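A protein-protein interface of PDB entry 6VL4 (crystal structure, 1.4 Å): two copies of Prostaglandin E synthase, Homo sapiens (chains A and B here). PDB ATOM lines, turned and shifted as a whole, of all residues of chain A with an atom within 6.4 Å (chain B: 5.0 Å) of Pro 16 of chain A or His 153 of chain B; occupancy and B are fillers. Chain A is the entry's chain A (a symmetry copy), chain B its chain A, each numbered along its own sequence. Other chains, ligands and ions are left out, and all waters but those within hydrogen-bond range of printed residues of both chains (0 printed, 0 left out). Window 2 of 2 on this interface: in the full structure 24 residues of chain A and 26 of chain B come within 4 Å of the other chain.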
ATOM      1  N   SER A  12     -10.419 -17.315  16.871  1.00  0.00           N
ATOM      2  CA  SER A  12      -9.209 -17.648  16.065  1.00  0.00           C
ATOM      3  C   SER A  12      -9.356 -17.092  14.648  1.00  0.00           C
ATOM      4  O   SER A  12     -10.397 -17.287  14.021  1.00  0.00           O
ATOM      5  CB  SER A  12      -8.965 -19.135  16.054  1.00  0.00           C
ATOM      6  N   PRO A  13      -8.331 -16.386  14.103  1.00  0.00           N
ATOM      7  CA  PRO A  13      -8.411 -15.798  12.762  1.00  0.00           C
ATOM      8  C   PRO A  13      -8.472 -16.807  11.615  1.00  0.00           C
ATOM      9  O   PRO A  13      -8.971 -16.484  10.537  1.00  0.00           O
ATOM     10  CB  PRO A  13      -7.123 -14.966  12.639  1.00  0.00           C
ATOM     11  CG  PRO A  13      -6.639 -14.799  14.064  1.00  0.00           C
ATOM     12  CD  PRO A  13      -7.051 -16.079  14.761  1.00  0.00           C
ATOM     13  N   ALA A  14      -7.969 -18.025  11.863  1.00  0.00           N
ATOM     14  CA  ALA A  14      -7.885 -19.071  10.854  1.00  0.00           C
ATOM     15  C   ALA A  14      -9.143 -19.940  10.854  1.00  0.00           C
ATOM     16  O   ALA A  14      -9.383 -20.673   9.896  1.00  0.00           O
ATOM     17  CB  ALA A  14      -6.647 -19.902  11.086  1.00  0.00           C
ATOM     18  N   LEU A  15      -9.935 -19.842  11.929  1.00  0.00           N
ATOM     19  CA  LEU A  15     -11.040 -20.755  12.191  1.00  0.00           C
ATOM     20  C   LEU A  15     -12.141 -20.657  11.131  1.00  0.00           C
ATOM     21  O   LEU A  15     -12.612 -21.699  10.683  1.00  0.00           O
ATOM     22  CB  LEU A  15     -11.567 -20.553  13.619  1.00  0.00           C
ATOM     23  CG  LEU A  15     -12.644 -21.533  14.090  1.00  0.00           C
ATOM     24  CD1 LEU A  15     -12.101 -22.954  14.186  1.00  0.00           C
ATOM     25  CD2 LEU A  15     -13.214 -21.102  15.434  1.00  0.00           C
ATOM     26  N   PRO A  16     -12.622 -19.455  10.706  1.00  0.00           N
ATOM     27  CA  PRO A  16     -13.632 -19.372   9.646  1.00  0.00           C
ATOM     28  C   PRO A  16     -13.266 -20.125   8.367  1.00  0.00           C
ATOM     29  O   PRO A  16     -14.104 -20.838   7.814  1.00  0.00           O
ATOM     30  CB  PRO A  16     -13.753 -17.864   9.373  1.00  0.00           C
ATOM     31  CG  PRO A  16     -13.375 -17.231  10.692  1.00  0.00           C
ATOM     32  CD  PRO A  16     -12.282 -18.123  11.241  1.00  0.00           C
ATOM     33  N   ALA A  17     -12.013 -19.966   7.914  1.00  0.00           N
ATOM     34  CA  ALA A  17     -11.518 -20.638   6.719  1.00  0.00           C
ATOM     35  C   ALA A  17     -11.511 -22.151   6.926  1.00  0.00           C
ATOM     36  O   ALA A  17     -11.899 -22.893   6.024  1.00  0.00           O
ATOM     37  CB  ALA A  17     -10.151 -20.126   6.346  1.00  0.00           C
ATOM     38  N   PHE A  18     -11.087 -22.594   8.119  1.00  0.00           N
ATOM     39  CA  PHE A  18     -11.077 -24.013   8.434  1.00  0.00           C
ATOM     40  C   PHE A  18     -12.493 -24.580   8.376  1.00  0.00           C
ATOM     41  O   PHE A  18     -12.706 -25.636   7.783  1.00  0.00           O
ATOM     42  CB  PHE A  18     -10.435 -24.317   9.792  1.00  0.00           C
ATOM     43  CG  PHE A  18     -10.748 -25.710  10.276  1.00  0.00           C
ATOM     44  CD1 PHE A  18     -10.132 -26.817   9.703  1.00  0.00           C
ATOM     45  CD2 PHE A  18     -11.707 -25.921  11.257  1.00  0.00           C
ATOM     46  CE1 PHE A  18     -10.448 -28.101  10.127  1.00  0.00           C
ATOM     47  CE2 PHE A  18     -12.034 -27.206  11.671  1.00  0.00           C
ATOM     48  CZ  PHE A  18     -11.396 -28.293  11.110  1.00  0.00           C
ATOM     49  N   LEU A  19     -13.450 -23.882   9.001  1.00  0.00           N
ATOM     50  CA  LEU A  19     -14.818 -24.369   9.101  1.00  0.00           C
ATOM     51  C   LEU A  19     -15.486 -24.402   7.729  1.00  0.00           C
ATOM     52  O   LEU A  19     -16.295 -25.291   7.468  1.00  0.00           O
ATOM     53  CB  LEU A  19     -15.617 -23.525  10.100  1.00  0.00           C
ATOM     54  CG  LEU A  19     -15.240 -23.676  11.575  1.00  0.00           C
ATOM     55  CD1 LEU A  19     -16.008 -22.674  12.423  1.00  0.00           C
ATOM     56  CD2 LEU A  19     -15.481 -25.093  12.081  1.00  0.00           C
ATOM     57  N   LEU A  20     -15.129 -23.445   6.860  1.00  0.00           N
ATOM     58  CA  LEU A  20     -15.651 -23.390   5.503  1.00  0.00           C
ATOM     59  C   LEU A  20     -15.179 -24.617   4.726  1.00  0.00           C
ATOM     60  O   LEU A  20     -15.998 -25.341   4.158  1.00  0.00           O
ATOM     61  CB  LEU A  20     -15.207 -22.082   4.831  1.00  0.00           C
ATOM     62  CG  LEU A  20     -15.773 -21.825   3.432  1.00  0.00           C
ATOM     63  CD1 LEU A  20     -17.119 -21.119   3.508  1.00  0.00           C
ATOM     64  CD2 LEU A  20     -14.797 -21.007   2.599  1.00  0.00           C
ATOM     65  N   CYS A  21     -13.861 -24.860   4.741  1.00  0.00           N
ATOM     66  CA  CYS A  21     -13.263 -25.939   3.967  1.00  0.00           C
ATOM     67  C   CYS A  21     -13.729 -27.298   4.481  1.00  0.00           C
ATOM     68  O   CYS A  21     -14.067 -28.169   3.682  1.00  0.00           O
ATOM     69  CB  CYS A  21     -11.742 -25.864   3.994  1.00  0.00           C
ATOM     70  SG  CYS A  21     -11.090 -24.433   3.094  1.00  0.00           S
ATOM     71  N   SER A  92      -5.992 -24.393  14.007  1.00  0.00           N
ATOM     72  CA  SER A  92      -6.647 -23.091  13.943  1.00  0.00           C
ATOM     73  C   SER A  92      -6.432 -22.284  15.225  1.00  0.00           C
ATOM     74  O   SER A  92      -6.399 -21.054  15.176  1.00  0.00           O
ATOM     75  CB  SER A  92      -8.115 -23.235  13.638  1.00  0.00           C
ATOM     76  OG  SER A  92      -8.314 -23.655  12.297  1.00  0.00           O
ATOM     77  N   GLU B 149     -22.250 -19.404   8.534  1.00  0.00           N
ATOM     78  CA  GLU B 149     -21.561 -18.747   9.634  1.00  0.00           C
ATOM     79  C   GLU B 149     -20.084 -18.578   9.287  1.00  0.00           C
ATOM     80  O   GLU B 149     -19.525 -17.502   9.476  1.00  0.00           O
ATOM     81  CB  GLU B 149     -21.760 -19.511  10.946  1.00  0.00           C
ATOM     82  CG  GLU B 149     -23.132 -19.312  11.564  1.00  0.00           C
ATOM     83  CD  GLU B 149     -23.533 -17.863  11.795  1.00  0.00           C
ATOM     84  OE1 GLU B 149     -24.688 -17.516  11.480  1.00  0.00           O
ATOM     85  OE2 GLU B 149     -22.691 -17.087  12.290  1.00  0.00           O
ATOM     86  N   ALA B 150     -19.465 -19.647   8.768  1.00  0.00           N
ATOM     87  CA  ALA B 150     -18.060 -19.629   8.390  1.00  0.00           C
ATOM     88  C   ALA B 150     -17.805 -18.598   7.291  1.00  0.00           C
ATOM     89  O   ALA B 150     -16.893 -17.783   7.416  1.00  0.00           O
ATOM     90  CB  ALA B 150     -17.604 -21.010   7.979  1.00  0.00           C
ATOM     91  N   ALA B 151     -18.633 -18.626   6.236  1.00  0.00           N
ATOM     92  CA  ALA B 151     -18.468 -17.767   5.071  1.00  0.00           C
ATOM     93  C   ALA B 151     -18.570 -16.291   5.455  1.00  0.00           C
ATOM     94  O   ALA B 151     -17.807 -15.471   4.946  1.00  0.00           O
ATOM     95  CB  ALA B 151     -19.474 -18.126   4.005  1.00  0.00           C
ATOM     96  N   ARG B 152     -19.492 -15.972   6.373  1.00  0.00           N
ATOM     97  CA  ARG B 152     -19.777 -14.587   6.720  1.00  0.00           C
ATOM     98  C   ARG B 152     -18.698 -14.018   7.644  1.00  0.00           C
ATOM     99  O   ARG B 152     -18.624 -12.802   7.819  1.00  0.00           O
ATOM    100  CB  ARG B 152     -21.210 -14.444   7.249  1.00  0.00           C
ATOM    101  CG  ARG B 152     -21.404 -14.805   8.715  1.00  0.00           C
ATOM    102  CD  ARG B 152     -22.859 -14.662   9.117  1.00  0.00           C
ATOM    103  NE  ARG B 152     -23.036 -14.681  10.562  1.00  0.00           N
ATOM    104  CZ  ARG B 152     -22.876 -13.636  11.372  1.00  0.00           C
ATOM    105  NH1 ARG B 152     -22.637 -12.433  10.877  1.00  0.00           N
ATOM    106  NH2 ARG B 152     -22.966 -13.799  12.680  1.00  0.00           N
ATOM    107  N   HIS B 153     -17.855 -14.901   8.204  1.00  0.00           N
ATOM    108  CA  HIS B 153     -16.810 -14.513   9.141  1.00  0.00           C
ATOM    109  C   HIS B 153     -15.445 -14.470   8.455  1.00  0.00           C
ATOM    110  O   HIS B 153     -14.431 -14.202   9.104  1.00  0.00           O
ATOM    111  CB  HIS B 153     -16.824 -15.431  10.372  1.00  0.00           C
ATOM    112  CG  HIS B 153     -17.805 -15.023  11.419  1.00  0.00           C
ATOM    113  ND1 HIS B 153     -19.069 -15.571  11.505  1.00  0.00           N
ATOM    114  CD2 HIS B 153     -17.714 -14.129  12.427  1.00  0.00           C
ATOM    115  CE1 HIS B 153     -19.716 -15.032  12.517  1.00  0.00           C
ATOM    116  NE2 HIS B 153     -18.904 -14.143  13.099  1.00  0.00           N
ATOM    117  N   LEU B 154     -15.425 -14.720   7.138  1.00  0.00           N
ATOM    118  CA  LEU B 154     -14.187 -14.730   6.369  1.00  0.00           C
ATOM    119  C   LEU B 154     -13.603 -13.313   6.278  1.00  0.00           C
ATOM    120  O   LEU B 154     -14.316 -12.311   6.304  1.00  0.00           O
ATOM    121  CB  LEU B 154     -14.442 -15.307   4.971  1.00  0.00           C
ATOM    122  CG  LEU B 154     -14.567 -16.828   4.875  1.00  0.00           C
ATOM    123  CD1 LEU B 154     -15.043 -17.238   3.490  1.00  0.00           C
ATOM    124  CD2 LEU B 154     -13.248 -17.519   5.203  1.00  0.00           C
ATOM    125  OXT LEU B 154     -12.386 -13.151   6.177  1.00  0.00           O
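O of Pro 16 of chain A touches CB of Ala 150 of chain B, 3.5 Å away. Pro 16 of chain A touches His 153 of chain B. N of Ala 17 of chain A touches CD2 of Leu 154 of chain B, 3.9 Å away. Leu 19 of chain A touches Ala 150 of chain B. Ala 150 of chain B touches Leu 20 of chain A. Ala 151 of chain B touches Leu 20 of chain A (CB to CD1, 3.8 Å). CD2 of Leu 20 of chain A touches CD1 of Leu 154 of chain B, 3.9 Å away.
The backbone carbonyl oxygen (O) of Ala 17 of chain A is in hydrogen-bond range of the side-chain sulfur (SG) of Cys 21 of chain A, at 3.4 Å. The backbone carbonyl oxygen (O) of Glu 149 of chain B lies within hydrogen-bond range of a ring nitrogen (ND1) of His 153 of chain B, at 2.8 Å.
No position is printed for both chains. Of the 7 pairs that touch across the chains among the printed residues, none has its exchanged pair printed and touching as well.
Printed residues of chain B within 4 Å of Pro 16 of chain A: Ala 150 and His 153. Of the printed residues of chain B, Ala 17 of chain A touches Leu 154. Of the printed residues of chain A, Leu 154 of chain B touches Ala 17 (3.9 Å) and Leu 20 (3.9 Å). Printed residues of chain A within 4 Å of Ala 151 of chain B: Leu 20 (3.8 Å). Leu 15 of chain A touches none of the printed residues of chain B. Pro 13 of chain A touches none of the printed residues of chain B.
Printed residues of chain A that touch a printed residue of chain B: Pro 16, Ala 17, Leu 19 and Leu 20. Hydrophobic or aromatic side chains of chain A that line the printed part of chain B: Pro 16, Leu 19 and Leu 20. Hydrophobic or aromatic side chains of chain B within 4 Å of the printed part of chain A: Ala 150, Ala 151, His 153 and Leu 154. Among the printed residues, 7 pairs touch across the chains. Among the printed residues, no Asp or Glu carboxylate lies within 4 Å of a Lys or Arg side-chain nitrogen of the other chain.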
